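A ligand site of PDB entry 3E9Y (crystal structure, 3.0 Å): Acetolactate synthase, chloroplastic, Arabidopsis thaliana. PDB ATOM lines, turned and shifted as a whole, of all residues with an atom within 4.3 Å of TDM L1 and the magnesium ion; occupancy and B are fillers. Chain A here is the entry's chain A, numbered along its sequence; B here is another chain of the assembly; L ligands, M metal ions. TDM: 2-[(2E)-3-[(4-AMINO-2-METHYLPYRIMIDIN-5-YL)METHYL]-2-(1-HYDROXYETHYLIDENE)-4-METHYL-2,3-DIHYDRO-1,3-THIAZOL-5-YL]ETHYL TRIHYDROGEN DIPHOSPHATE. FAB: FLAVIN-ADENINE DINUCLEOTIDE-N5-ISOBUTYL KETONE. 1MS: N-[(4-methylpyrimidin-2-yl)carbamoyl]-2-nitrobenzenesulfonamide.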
ATOM      1  N   VAL A 399      -1.687  -9.193 -18.887  1.00  0.00           N
ATOM      2  CA  VAL A 399      -2.832  -9.043 -18.000  1.00  0.00           C
ATOM      3  C   VAL A 399      -3.144 -10.348 -17.276  1.00  0.00           C
ATOM      4  O   VAL A 399      -3.228 -11.411 -17.896  1.00  0.00           O
ATOM      5  CB  VAL A 399      -4.077  -8.538 -18.769  1.00  0.00           C
ATOM      6  CG1 VAL A 399      -5.331  -8.674 -17.922  1.00  0.00           C
ATOM      7  CG2 VAL A 399      -3.876  -7.100 -19.154  1.00  0.00           C
ATOM      8  N   GLY A 400      -3.328 -10.257 -15.958  1.00  0.00           N
ATOM      9  CA  GLY A 400      -3.677 -11.411 -15.150  1.00  0.00           C
ATOM     10  C   GLY A 400      -2.838 -11.528 -13.899  1.00  0.00           C
ATOM     11  O   GLY A 400      -2.256 -10.534 -13.431  1.00  0.00           O
ATOM     12  N   GLN A 401      -2.778 -12.742 -13.356  1.00  0.00           N
ATOM     13  CA  GLN A 401      -2.064 -13.005 -12.107  1.00  0.00           C
ATOM     14  C   GLN A 401      -0.681 -12.367 -12.089  1.00  0.00           C
ATOM     15  O   GLN A 401      -0.323 -11.687 -11.139  1.00  0.00           O
ATOM     16  CB  GLN A 401      -1.929 -14.500 -11.872  1.00  0.00           C
ATOM     17  CG  GLN A 401      -3.223 -15.222 -11.562  1.00  0.00           C
ATOM     18  CD  GLN A 401      -3.004 -16.672 -11.190  1.00  0.00           C
ATOM     19  OE1 GLN A 401      -2.177 -17.362 -11.805  1.00  0.00           O
ATOM     20  NE2 GLN A 401      -3.723 -17.146 -10.184  1.00  0.00           N
ATOM     21  N   HIS A 402       0.089 -12.580 -13.155  1.00  0.00           N
ATOM     22  CA  HIS A 402       1.458 -12.100 -13.206  1.00  0.00           C
ATOM     23  C   HIS A 402       1.517 -10.564 -13.142  1.00  0.00           C
ATOM     24  O   HIS A 402       2.472 -10.004 -12.615  1.00  0.00           O
ATOM     25  CB  HIS A 402       2.182 -12.631 -14.448  1.00  0.00           C
ATOM     26  CG  HIS A 402       1.765 -11.973 -15.723  1.00  0.00           C
ATOM     27  ND1 HIS A 402       0.586 -12.278 -16.368  1.00  0.00           N
ATOM     28  CD2 HIS A 402       2.371 -11.018 -16.476  1.00  0.00           C
ATOM     29  CE1 HIS A 402       0.477 -11.537 -17.466  1.00  0.00           C
ATOM     30  NE2 HIS A 402       1.548 -10.776 -17.548  1.00  0.00           N
ATOM     31  N   GLY A 425      -7.467  -3.632 -19.832  1.00  0.00           N
ATOM     32  CA  GLY A 425      -6.851  -4.897 -19.431  1.00  0.00           C
ATOM     33  C   GLY A 425      -6.617  -5.832 -20.607  1.00  0.00           C
ATOM     34  O   GLY A 425      -7.057  -6.984 -20.589  1.00  0.00           O
ATOM     35  N   MET A 427      -4.666  -8.251 -23.056  1.00  0.00           N
ATOM     36  CA  MET A 427      -3.560  -9.205 -23.157  1.00  0.00           C
ATOM     37  C   MET A 427      -2.704  -8.925 -24.399  1.00  0.00           C
ATOM     38  O   MET A 427      -3.173  -8.319 -25.367  1.00  0.00           O
ATOM     39  CB  MET A 427      -4.087 -10.634 -23.178  1.00  0.00           C
ATOM     40  CG  MET A 427      -4.533 -11.161 -21.836  1.00  0.00           C
ATOM     41  SD  MET A 427      -5.365 -12.745 -21.996  1.00  0.00           S
ATOM     42  CE  MET A 427      -4.023 -13.830 -22.437  1.00  0.00           C
ATOM     43  N   GLY A 451       2.993 -13.156 -19.051  1.00  0.00           N
ATOM     44  CA  GLY A 451       2.436 -14.494 -18.813  1.00  0.00           C
ATOM     45  C   GLY A 451       2.364 -15.254 -20.122  1.00  0.00           C
ATOM     46  O   GLY A 451       2.305 -14.647 -21.181  1.00  0.00           O
ATOM     47  N   ASP A 452       2.370 -16.583 -20.060  1.00  0.00           N
ATOM     48  CA  ASP A 452       2.425 -17.401 -21.280  1.00  0.00           C
ATOM     49  C   ASP A 452       1.198 -17.209 -22.166  1.00  0.00           C
ATOM     50  O   ASP A 452       1.283 -17.293 -23.396  1.00  0.00           O
ATOM     51  CB  ASP A 452       2.698 -18.880 -20.986  1.00  0.00           C
ATOM     52  CG  ASP A 452       1.581 -19.539 -20.196  1.00  0.00           C
ATOM     53  OD1 ASP A 452       1.160 -18.984 -19.159  1.00  0.00           O
ATOM     54  OD2 ASP A 452       1.132 -20.631 -20.616  1.00  0.00           O
ATOM     55  N   GLY A 453       0.052 -16.958 -21.536  1.00  0.00           N
ATOM     56  CA  GLY A 453      -1.163 -16.622 -22.282  1.00  0.00           C
ATOM     57  C   GLY A 453      -1.017 -15.328 -23.060  1.00  0.00           C
ATOM     58  O   GLY A 453      -1.303 -15.280 -24.258  1.00  0.00           O
ATOM     59  N   SER A 454      -0.575 -14.286 -22.367  1.00  0.00           N
ATOM     60  CA  SER A 454      -0.410 -12.958 -22.953  1.00  0.00           C
ATOM     61  C   SER A 454       0.752 -12.908 -23.932  1.00  0.00           C
ATOM     62  O   SER A 454       0.635 -12.319 -25.003  1.00  0.00           O
ATOM     63  CB  SER A 454      -0.230 -11.903 -21.871  1.00  0.00           C
ATOM     64  OG  SER A 454      -1.323 -11.909 -20.971  1.00  0.00           O
ATOM     65  N   MET A 457       0.214 -14.137 -27.592  1.00  0.00           N
ATOM     66  CA  MET A 457      -0.685 -13.294 -28.400  1.00  0.00           C
ATOM     67  C   MET A 457       0.050 -12.359 -29.342  1.00  0.00           C
ATOM     68  O   MET A 457      -0.395 -12.142 -30.477  1.00  0.00           O
ATOM     69  CB  MET A 457      -1.598 -12.453 -27.502  1.00  0.00           C
ATOM     70  CG  MET A 457      -2.597 -13.239 -26.715  1.00  0.00           C
ATOM     71  SD  MET A 457      -4.004 -12.187 -26.377  1.00  0.00           S
ATOM     72  CE  MET A 457      -5.227 -13.383 -25.840  1.00  0.00           C
ATOM     73  N   ASN A 479       2.994 -20.442 -16.266  1.00  0.00           N
ATOM     74  CA  ASN A 479       2.214 -21.359 -15.429  1.00  0.00           C
ATOM     75  C   ASN A 479       1.197 -22.216 -16.191  1.00  0.00           C
ATOM     76  O   ASN A 479       0.266 -22.774 -15.595  1.00  0.00           O
ATOM     77  CB  ASN A 479       1.554 -20.623 -14.248  1.00  0.00           C
ATOM     78  CG  ASN A 479       0.413 -19.701 -14.685  1.00  0.00           C
ATOM     79  OD1 ASN A 479       0.029 -19.651 -15.859  1.00  0.00           O
ATOM     80  ND2 ASN A 479      -0.140 -18.973 -13.724  1.00  0.00           N
ATOM     81  N   HIS A 481      -1.359 -21.827 -17.830  1.00  0.00           N
ATOM     82  CA  HIS A 481      -2.785 -21.524 -17.699  1.00  0.00           C
ATOM     83  C   HIS A 481      -3.096 -20.056 -17.901  1.00  0.00           C
ATOM     84  O   HIS A 481      -2.224 -19.193 -17.754  1.00  0.00           O
ATOM     85  CB  HIS A 481      -3.290 -21.926 -16.313  1.00  0.00           C
ATOM     86  CG  HIS A 481      -3.448 -23.397 -16.124  1.00  0.00           C
ATOM     87  ND1 HIS A 481      -2.409 -24.219 -15.743  1.00  0.00           N
ATOM     88  CD2 HIS A 481      -4.533 -24.200 -16.253  1.00  0.00           C
ATOM     89  CE1 HIS A 481      -2.836 -25.462 -15.650  1.00  0.00           C
ATOM     90  NE2 HIS A 481      -4.123 -25.477 -15.950  1.00  0.00           N
ATOM     91  N   LEU A 482      -4.351 -19.781 -18.253  1.00  0.00           N
ATOM     92  CA  LEU A 482      -4.921 -18.440 -18.112  1.00  0.00           C
ATOM     93  C   LEU A 482      -5.254 -18.258 -16.627  1.00  0.00           C
ATOM     94  O   LEU A 482      -6.397 -18.462 -16.199  1.00  0.00           O
ATOM     95  CB  LEU A 482      -6.174 -18.280 -18.980  1.00  0.00           C
ATOM     96  CG  LEU A 482      -6.010 -18.458 -20.490  1.00  0.00           C
ATOM     97  CD1 LEU A 482      -7.354 -18.438 -21.172  1.00  0.00           C
ATOM     98  CD2 LEU A 482      -5.091 -17.395 -21.055  1.00  0.00           C
ATOM     99  N   GLY A 483      -4.237 -17.889 -15.856  1.00  0.00           N
ATOM    100  CA  GLY A 483      -4.274 -17.911 -14.390  1.00  0.00           C
ATOM    101  C   GLY A 483      -5.382 -17.124 -13.719  1.00  0.00           C
ATOM    102  O   GLY A 483      -6.033 -17.639 -12.814  1.00  0.00           O
ATOM    103  N   MET A 484      -5.584 -15.880 -14.161  1.00  0.00           N
ATOM    104  CA  MET A 484      -6.595 -15.019 -13.564  1.00  0.00           C
ATOM    105  C   MET A 484      -7.987 -15.620 -13.682  1.00  0.00           C
ATOM    106  O   MET A 484      -8.788 -15.552 -12.740  1.00  0.00           O
ATOM    107  CB  MET A 484      -6.546 -13.622 -14.181  1.00  0.00           C
ATOM    108  CG  MET A 484      -7.380 -12.576 -13.446  1.00  0.00           C
ATOM    109  SD  MET A 484      -6.926 -12.410 -11.701  1.00  0.00           S
ATOM    110  CE  MET A 484      -5.521 -11.312 -11.830  1.00  0.00           C
ATOM    111  N   VAL A 485      -8.279 -16.212 -14.845  1.00  0.00           N
ATOM    112  CA  VAL A 485      -9.559 -16.871 -15.089  1.00  0.00           C
ATOM    113  C   VAL A 485      -9.647 -18.138 -14.249  1.00  0.00           C
ATOM    114  O   VAL A 485     -10.708 -18.452 -13.690  1.00  0.00           O
ATOM    115  CB  VAL A 485      -9.757 -17.199 -16.585  1.00  0.00           C
ATOM    116  CG1 VAL A 485     -11.196 -17.599 -16.865  1.00  0.00           C
ATOM    117  CG2 VAL A 485      -9.377 -15.997 -17.452  1.00  0.00           C
ATOM    118  N   LEU A 502      -3.451 -23.992 -21.101  1.00  0.00           N
ATOM    119  CA  LEU A 502      -2.773 -23.545 -22.317  1.00  0.00           C
ATOM    120  C   LEU A 502      -1.797 -24.568 -22.920  1.00  0.00           C
ATOM    121  O   LEU A 502      -1.325 -24.380 -24.042  1.00  0.00           O
ATOM    122  CB  LEU A 502      -2.065 -22.209 -22.087  1.00  0.00           C
ATOM    123  CG  LEU A 502      -2.928 -20.966 -21.837  1.00  0.00           C
ATOM    124  CD1 LEU A 502      -2.054 -19.838 -21.339  1.00  0.00           C
ATOM    125  CD2 LEU A 502      -3.688 -20.532 -23.084  1.00  0.00           C
ATOM    126  N   TYR B  32     -12.627 -17.802 -26.695  1.00  0.00           N
ATOM    127  CA  TYR B  32     -11.534 -17.483 -25.782  1.00  0.00           C
ATOM    128  C   TYR B  32     -12.118 -16.852 -24.513  1.00  0.00           C
ATOM    129  O   TYR B  32     -12.843 -15.865 -24.595  1.00  0.00           O
ATOM    130  CB  TYR B  32     -10.560 -16.516 -26.456  1.00  0.00           C
ATOM    131  CG  TYR B  32      -9.198 -16.468 -25.814  1.00  0.00           C
ATOM    132  CD1 TYR B  32      -8.150 -17.230 -26.315  1.00  0.00           C
ATOM    133  CD2 TYR B  32      -8.954 -15.658 -24.721  1.00  0.00           C
ATOM    134  CE1 TYR B  32      -6.890 -17.188 -25.722  1.00  0.00           C
ATOM    135  CE2 TYR B  32      -7.701 -15.602 -24.122  1.00  0.00           C
ATOM    136  CZ  TYR B  32      -6.675 -16.363 -24.628  1.00  0.00           C
ATOM    137  OH  TYR B  32      -5.450 -16.300 -24.024  1.00  0.00           O
ATOM    138  N   PRO B  33     -11.796 -17.430 -23.343  1.00  0.00           N
ATOM    139  CA  PRO B  33     -12.479 -17.041 -22.112  1.00  0.00           C
ATOM    140  C   PRO B  33     -11.921 -15.770 -21.458  1.00  0.00           C
ATOM    141  O   PRO B  33     -10.758 -15.402 -21.668  1.00  0.00           O
ATOM    142  CB  PRO B  33     -12.251 -18.246 -21.198  1.00  0.00           C
ATOM    143  CG  PRO B  33     -10.965 -18.813 -21.645  1.00  0.00           C
ATOM    144  CD  PRO B  33     -10.787 -18.479 -23.100  1.00  0.00           C
ATOM    145  N   GLY B  34     -12.781 -15.126 -20.675  1.00  0.00           N
ATOM    146  CA  GLY B  34     -12.431 -13.944 -19.913  1.00  0.00           C
ATOM    147  C   GLY B  34     -13.485 -13.643 -18.864  1.00  0.00           C
ATOM    148  O   GLY B  34     -14.521 -14.319 -18.801  1.00  0.00           O
ATOM    149  N   GLY B  35     -13.236 -12.625 -18.060  1.00  0.00           N
ATOM    150  CA  GLY B  35     -14.109 -12.249 -16.952  1.00  0.00           C
ATOM    151  C   GLY B  35     -15.592 -12.200 -17.271  1.00  0.00           C
ATOM    152  O   GLY B  35     -16.404 -12.810 -16.574  1.00  0.00           O
ATOM    153  N   GLU B  58      -7.949 -13.899 -30.147  1.00  0.00           N
ATOM    154  CA  GLU B  58      -9.331 -13.921 -30.629  1.00  0.00           C
ATOM    155  C   GLU B  58      -9.528 -13.502 -32.088  1.00  0.00           C
ATOM    156  O   GLU B  58     -10.574 -13.804 -32.679  1.00  0.00           O
ATOM    157  CB  GLU B  58     -10.246 -13.133 -29.677  1.00  0.00           C
ATOM    158  CG  GLU B  58      -9.474 -12.283 -28.698  1.00  0.00           C
ATOM    159  CD  GLU B  58      -9.889 -12.538 -27.269  1.00  0.00           C
ATOM    160  OE1 GLU B  58      -9.045 -12.309 -26.369  1.00  0.00           O
ATOM    161  OE2 GLU B  58     -11.035 -12.959 -27.022  1.00  0.00           O
ATOM    162  N   THR B  81     -14.783 -12.421 -24.545  1.00  0.00           N
ATOM    163  CA  THR B  81     -15.109 -11.626 -23.370  1.00  0.00           C
ATOM    164  C   THR B  81     -15.345 -10.154 -23.747  1.00  0.00           C
ATOM    165  O   THR B  81     -15.243  -9.768 -24.917  1.00  0.00           O
ATOM    166  CB  THR B  81     -14.020 -11.756 -22.276  1.00  0.00           C
ATOM    167  OG1 THR B  81     -14.525 -11.215 -21.037  1.00  0.00           O
ATOM    168  CG2 THR B  81     -12.726 -11.029 -22.653  1.00  0.00           C
ATOM    169  N   PRO B  84     -11.207  -5.961 -24.310  1.00  0.00           N
ATOM    170  CA  PRO B  84     -10.148  -6.341 -25.231  1.00  0.00           C
ATOM    171  C   PRO B  84     -10.489  -7.601 -26.020  1.00  0.00           C
ATOM    172  O   PRO B  84     -10.079  -7.727 -27.184  1.00  0.00           O
ATOM    173  CB  PRO B  84      -8.943  -6.578 -24.301  1.00  0.00           C
ATOM    174  CG  PRO B  84      -9.554  -6.892 -22.976  1.00  0.00           C
ATOM    175  CD  PRO B  84     -10.795  -6.061 -22.904  1.00  0.00           C
ATOM    176  N   GLY B  85     -11.225  -8.521 -25.413  1.00  0.00           N
ATOM    177  CA  GLY B  85     -11.710  -9.709 -26.105  1.00  0.00           C
ATOM    178  C   GLY B  85     -12.547  -9.294 -27.294  1.00  0.00           C
ATOM    179  O   GLY B  85     -12.286  -9.701 -28.423  1.00  0.00           O
ATOM    180  N   ASN B  88     -10.827  -7.336 -30.273  1.00  0.00           N
ATOM    181  CA  ASN B  88      -9.954  -8.188 -31.080  1.00  0.00           C
ATOM    182  C   ASN B  88     -10.686  -8.952 -32.179  1.00  0.00           C
ATOM    183  O   ASN B  88     -10.059  -9.546 -33.054  1.00  0.00           O
ATOM    184  CB  ASN B  88      -9.148  -9.140 -30.197  1.00  0.00           C
ATOM    185  CG  ASN B  88      -7.994  -8.461 -29.501  1.00  0.00           C
ATOM    186  OD1 ASN B  88      -7.524  -8.926 -28.455  1.00  0.00           O
ATOM    187  ND2 ASN B  88      -7.503  -7.360 -30.072  1.00  0.00           N
ATOM    188  N   PHE B 120     -14.583  -1.801 -15.611  1.00  0.00           N
ATOM    189  CA  PHE B 120     -13.489  -2.717 -15.888  1.00  0.00           C
ATOM    190  C   PHE B 120     -13.771  -3.534 -17.145  1.00  0.00           C
ATOM    191  O   PHE B 120     -14.769  -4.270 -17.211  1.00  0.00           O
ATOM    192  CB  PHE B 120     -13.265  -3.638 -14.685  1.00  0.00           C
ATOM    193  CG  PHE B 120     -12.152  -4.639 -14.870  1.00  0.00           C
ATOM    194  CD1 PHE B 120     -10.841  -4.217 -15.005  1.00  0.00           C
ATOM    195  CD2 PHE B 120     -12.435  -5.994 -14.892  1.00  0.00           C
ATOM    196  CE1 PHE B 120      -9.813  -5.136 -15.178  1.00  0.00           C
ATOM    197  CE2 PHE B 120     -11.419  -6.928 -15.055  1.00  0.00           C
ATOM    198  CZ  PHE B 120     -10.097  -6.500 -15.196  1.00  0.00           C
ATOM    199  N   GLN B 121     -12.890  -3.383 -18.135  1.00  0.00           N
ATOM    200  CA  GLN B 121     -12.996  -4.067 -19.431  1.00  0.00           C
ATOM    201  C   GLN B 121     -14.295  -3.740 -20.174  1.00  0.00           C
ATOM    202  O   GLN B 121     -14.924  -4.629 -20.747  1.00  0.00           O
ATOM    203  CB  GLN B 121     -12.826  -5.578 -19.276  1.00  0.00           C
ATOM    204  CG  GLN B 121     -11.555  -5.997 -18.579  1.00  0.00           C
ATOM    205  CD  GLN B 121     -11.200  -7.453 -18.808  1.00  0.00           C
ATOM    206  OE1 GLN B 121     -11.996  -8.346 -18.525  1.00  0.00           O
ATOM    207  NE2 GLN B 121      -9.988  -7.686 -19.319  1.00  0.00           N
HETATM  208  O1A TDM L   1      -0.981 -16.618 -18.750  1.00  0.00           O
HETATM  209  PA  TDM L   1      -1.655 -15.293 -18.710  1.00  0.00           P
HETATM  210  O2A TDM L   1      -1.032 -14.327 -19.801  1.00  0.00           O
HETATM  211  O3A TDM L   1      -1.447 -14.511 -17.301  1.00  0.00           O
HETATM  212  PB  TDM L   1      -1.600 -15.193 -15.863  1.00  0.00           P
HETATM  213  O2B TDM L   1      -0.509 -14.802 -14.933  1.00  0.00           O
HETATM  214  O3B TDM L   1      -3.051 -14.778 -15.285  1.00  0.00           O
HETATM  215  O1B TDM L   1      -1.681 -16.794 -16.040  1.00  0.00           O
HETATM  216  O7  TDM L   1      -3.231 -15.338 -19.024  1.00  0.00           O
HETATM  217  C7  TDM L   1      -4.094 -14.216 -18.805  1.00  0.00           C
HETATM  218  C6  TDM L   1      -5.442 -14.741 -18.325  1.00  0.00           C
HETATM  219  C5  TDM L   1      -6.581 -13.738 -18.486  1.00  0.00           C
HETATM  220  S1  TDM L   1      -6.834 -12.505 -17.308  1.00  0.00           S
HETATM  221  C2  TDM L   1      -8.212 -11.810 -18.061  1.00  0.00           C
HETATM  222  C27 TDM L   1      -8.904 -10.763 -17.593  1.00  0.00           C
HETATM  223  C29 TDM L   1      -8.506 -10.081 -16.281  1.00  0.00           C
HETATM  224  O28 TDM L   1     -10.110 -10.221 -18.364  1.00  0.00           O
HETATM  225  N3  TDM L   1      -8.449 -12.635 -19.348  1.00  0.00           N
HETATM  226  C4  TDM L   1      -7.549 -13.636 -19.502  1.00  0.00           C
HETATM  227  CM4 TDM L   1      -7.571 -14.595 -20.693  1.00  0.00           C
HETATM  228  C7' TDM L   1      -9.532 -12.332 -20.312  1.00  0.00           C
HETATM  229  C5' TDM L   1      -8.900 -11.617 -21.530  1.00  0.00           C
HETATM  230  C4' TDM L   1      -8.162 -10.421 -21.496  1.00  0.00           C
HETATM  231  N4' TDM L   1      -7.946  -9.773 -20.357  1.00  0.00           N
HETATM  232  N3' TDM L   1      -7.652  -9.905 -22.630  1.00  0.00           N
HETATM  233  C2' TDM L   1      -7.838 -10.519 -23.812  1.00  0.00           C
HETATM  234  CM2 TDM L   1      -7.247  -9.906 -25.080  1.00  0.00           C
HETATM  235  N1' TDM L   1      -8.539 -11.667 -23.873  1.00  0.00           N
HETATM  236  C6' TDM L   1      -9.064 -12.213 -22.790  1.00  0.00           C
HETATM  237  PA  FAB L   2      -6.729   6.493 -14.390  1.00  0.00           P
HETATM  238  O1A FAB L   2      -5.260   6.561 -14.189  1.00  0.00           O
HETATM  239  O2A FAB L   2      -7.315   5.546 -15.379  1.00  0.00           O
HETATM  240  O5B FAB L   2      -7.222   7.963 -14.756  1.00  0.00           O
HETATM  241  C5B FAB L   2      -6.644   9.081 -14.093  1.00  0.00           C
HETATM  242  C4B FAB L   2      -7.686  10.098 -13.635  1.00  0.00           C
HETATM  243  O4B FAB L   2      -6.901  11.270 -13.352  1.00  0.00           O
HETATM  244  C3B FAB L   2      -8.674  10.477 -14.751  1.00  0.00           C
HETATM  245  O3B FAB L   2      -9.963  10.722 -14.160  1.00  0.00           O
HETATM  246  C2B FAB L   2      -8.090  11.748 -15.355  1.00  0.00           C
HETATM  247  O2B FAB L   2      -9.147  12.619 -15.782  1.00  0.00           O
HETATM  248  C1B FAB L   2      -7.370  12.379 -14.159  1.00  0.00           C
HETATM  249  N9A FAB L   2      -6.161  13.190 -14.470  1.00  0.00           N
HETATM  250  C8A FAB L   2      -5.266  12.940 -15.422  1.00  0.00           C
HETATM  251  N7A FAB L   2      -4.315  13.882 -15.400  1.00  0.00           N
HETATM  252  C5A FAB L   2      -4.611  14.725 -14.416  1.00  0.00           C
HETATM  253  C6A FAB L   2      -3.976  15.867 -13.941  1.00  0.00           C
HETATM  254  N6A FAB L   2      -2.896  16.325 -14.569  1.00  0.00           N
HETATM  255  N1A FAB L   2      -4.449  16.537 -12.802  1.00  0.00           N
HETATM  256  C2A FAB L   2      -5.642  16.082 -12.048  1.00  0.00           C
HETATM  257  N3A FAB L   2      -6.349  14.977 -12.749  1.00  0.00           N
HETATM  258  C4A FAB L   2      -5.778  14.276 -13.823  1.00  0.00           C
HETATM  259  N1  FAB L   2      -6.427  -1.095 -10.117  1.00  0.00           N
HETATM  260  C2  FAB L   2      -6.257  -0.900  -8.740  1.00  0.00           C
HETATM  261  O2  FAB L   2      -5.986   0.222  -8.309  1.00  0.00           O
HETATM  262  N3  FAB L   2      -6.399  -1.974  -7.849  1.00  0.00           N
HETATM  263  C4  FAB L   2      -6.703  -3.249  -8.346  1.00  0.00           C
HETATM  264  O4  FAB L   2      -6.825  -4.196  -7.562  1.00  0.00           O
HETATM  265  C4X FAB L   2      -6.883  -3.442  -9.721  1.00  0.00           C
HETATM  266  N5  FAB L   2      -7.186  -4.708 -10.221  1.00  0.00           N
HETATM  267  C5X FAB L   2      -6.974  -4.973 -11.579  1.00  0.00           C
HETATM  268  C6  FAB L   2      -6.896  -6.286 -12.035  1.00  0.00           C
HETATM  269  C7  FAB L   2      -6.669  -6.537 -13.380  1.00  0.00           C
HETATM  270  C7M FAB L   2      -6.599  -7.996 -13.823  1.00  0.00           C
HETATM  271  C8  FAB L   2      -6.533  -5.479 -14.285  1.00  0.00           C
HETATM  272  C8M FAB L   2      -6.282  -5.697 -15.780  1.00  0.00           C
HETATM  273  C9  FAB L   2      -6.609  -4.162 -13.820  1.00  0.00           C
HETATM  274  C9A FAB L   2      -6.846  -3.909 -12.473  1.00  0.00           C
HETATM  275  N10 FAB L   2      -6.907  -2.588 -11.991  1.00  0.00           N
HETATM  276  C10 FAB L   2      -6.749  -2.363 -10.601  1.00  0.00           C
HETATM  277  C1' FAB L   2      -7.005  -1.464 -12.951  1.00  0.00           C
HETATM  278  C2D FAB L   2      -8.272  -0.628 -12.797  1.00  0.00           C
HETATM  279  O2' FAB L   2      -9.331  -1.204 -13.556  1.00  0.00           O
HETATM  280  C3D FAB L   2      -8.034   0.787 -13.303  1.00  0.00           C
HETATM  281  O3D FAB L   2      -7.155   0.742 -14.427  1.00  0.00           O
HETATM  282  C4D FAB L   2      -7.429   1.716 -12.246  1.00  0.00           C
HETATM  283  O4' FAB L   2      -7.997   1.451 -10.973  1.00  0.00           O
HETATM  284  C5D FAB L   2      -7.706   3.172 -12.596  1.00  0.00           C
HETATM  285  O5' FAB L   2      -6.614   4.002 -12.215  1.00  0.00           O
HETATM  286  P   FAB L   2      -6.901   5.516 -11.717  1.00  0.00           P
HETATM  287  O1P FAB L   2      -8.016   5.492 -10.738  1.00  0.00           O
HETATM  288  O2P FAB L   2      -5.595   6.116 -11.369  1.00  0.00           O
HETATM  289  O3P FAB L   2      -7.511   6.250 -13.005  1.00  0.00           O
HETATM  290  O8  1MS L   3     -16.460  -7.907 -16.854  1.00  0.00           O
HETATM  291  N7  1MS L   3     -17.013  -8.076 -15.554  1.00  0.00           N
HETATM  292  O9  1MS L   3     -17.384  -9.384 -15.176  1.00  0.00           O
HETATM  293  C1  1MS L   3     -17.168  -7.003 -14.757  1.00  0.00           C
HETATM  294  C6  1MS L   3     -16.768  -5.784 -15.285  1.00  0.00           C
HETATM  295  C5  1MS L   3     -16.851  -4.582 -14.598  1.00  0.00           C
HETATM  296  C4  1MS L   3     -17.350  -4.451 -13.294  1.00  0.00           C
HETATM  297  C3  1MS L   3     -17.831  -5.737 -12.612  1.00  0.00           C
HETATM  298  C2  1MS L   3     -17.685  -7.011 -13.451  1.00  0.00           C
HETATM  299  S10 1MS L   3     -18.253  -8.470 -12.637  1.00  0.00           S
HETATM  300  O11 1MS L   3     -18.373  -8.197 -11.174  1.00  0.00           O
HETATM  301  O12 1MS L   3     -19.607  -8.818 -13.157  1.00  0.00           O
HETATM  302  N13 1MS L   3     -17.272  -9.800 -12.819  1.00  0.00           N
HETATM  303  C14 1MS L   3     -15.941  -9.656 -12.667  1.00  0.00           C
HETATM  304  O15 1MS L   3     -15.444  -8.661 -12.146  1.00  0.00           O
HETATM  305  N16 1MS L   3     -15.236 -10.692 -13.132  1.00  0.00           N
HETATM  306  C18 1MS L   3     -13.892 -10.822 -13.111  1.00  0.00           C
HETATM  307  N17 1MS L   3     -13.073  -9.826 -12.714  1.00  0.00           N
HETATM  308  C23 1MS L   3     -11.753  -9.959 -12.708  1.00  0.00           C
HETATM  309  C22 1MS L   3     -11.145 -11.147 -13.124  1.00  0.00           C
HETATM  310  C20 1MS L   3     -11.947 -12.196 -13.538  1.00  0.00           C
HETATM  311  C21 1MS L   3     -11.382 -13.392 -13.962  1.00  0.00           C
HETATM  312  N19 1MS L   3     -13.345 -12.041 -13.544  1.00  0.00           N
HETATM  313 MG    MG M   1      -0.211 -17.998 -17.411  1.00  0.00          MG
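The magnesium ion is bound by O1A of TDM L1 (2.1 Å). The side-chain amide oxygen (OD1) of Asn 479 is bound to the magnesium ion (2.3 Å). The magnesium ion is bound by O1B of TDM L1 (2.3 Å). The magnesium ion is bound by O of His 481, at 2.4 Å. The magnesium ion is bound by OD1 of Asp 452, at 2.4 Å.
The side-chain hydroxyl of Ser 454 sits at hydrogen-bond distance from an oxygen (O2A) of TDM L1 (2.7 Å). O28 of TDM L1 lies within hydrogen-bond range of OE1 of Gln 121 of chain B, 2.7 Å away. The backbone NH of His 402 lies within hydrogen-bond range of an oxygen (O2B) of TDM L1 (2.9 Å). The side-chain carboxylate (OE1) of Glu 58 of chain B lies within hydrogen-bond range of a nitrogen (N1') of TDM L1. N of Met 427 is in hydrogen-bond range of N3' of TDM L1 (3.4 Å). An oxygen (O2A) of TDM L1 is in hydrogen-bond range of the backbone NH (N) of Ser 454. O2B of TDM L1 lies within hydrogen-bond range of ND1 of His 402 (3.1 Å). A nitrogen (N4') of TDM L1 lies within hydrogen-bond range of the backbone carbonyl oxygen (O) of Gly 425 (2.9 Å). The backbone NH (N) of Gly 453 is in hydrogen-bond range of an oxygen (O2A) of TDM L1 (3.3 Å). An oxygen (O3B) of TDM L1 lies within hydrogen-bond range of the backbone NH (N) of Gly 483 (3.4 Å). The backbone NH (N) of Gln 401 is in hydrogen-bond range of an oxygen (O3B) of TDM L1 (2.8 Å). N of Met 484 sits at hydrogen-bond distance from O3B of TDM L1, 3.0 Å away.
Residues that only touch TDM L1: Val 399, Gly 34 of chain B, Gly 400, Pro 33 of chain B, Leu 482, Asn 88 of chain B, Gly 451, Tyr 32 of chain B, Pro 84 of chain B, Val 485, Thr 81 of chain B and Gly 35 of chain B. 25 residues have an atom within 4 Å of TDM L1: Val 399, Gly 400, Gln 401, His 402, Gly 425, Met 427, Gly 451, Asp 452, Gly 453, Ser 454, Asn 479, His 481, Leu 482, Gly 483, Met 484, Val 485, Tyr 32 of chain B, Pro 33 of chain B, Gly 34 of chain B, Gly 35 of chain B, Glu 58 of chain B, Thr 81 of chain B, Pro 84 of chain B, Asn 88 of chain B and Gln 121 of chain B. The nearest printed residue that does not touch TDM L1 is Phe 120 of chain B (4.1 Å).
Of the 29 residues printed, 3 come within 4 Å of the magnesium ion. The nearest printed residue that does not touch the magnesium ion is Gly 453 (4.3 Å).
The side-chain amide nitrogen (NE2) of Gln 121 of chain B sits at hydrogen-bond distance from the backbone carbonyl oxygen (O) of Gly 425, at 3.3 Å. OG of Ser 454 lies within hydrogen-bond range of N of Val 399. The side-chain amide oxygen of Asn 88 of chain B sits close to the backbone carbonyl oxygen of Pro 84 of chain B (3.1 Å). NE2 of His 402 sits at hydrogen-bond distance from N of Gly 451. The side-chain amide nitrogen (ND2) of Asn 479 lies within hydrogen-bond range of the side-chain amide oxygen (OE1) of Gln 401 (3.2 Å).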
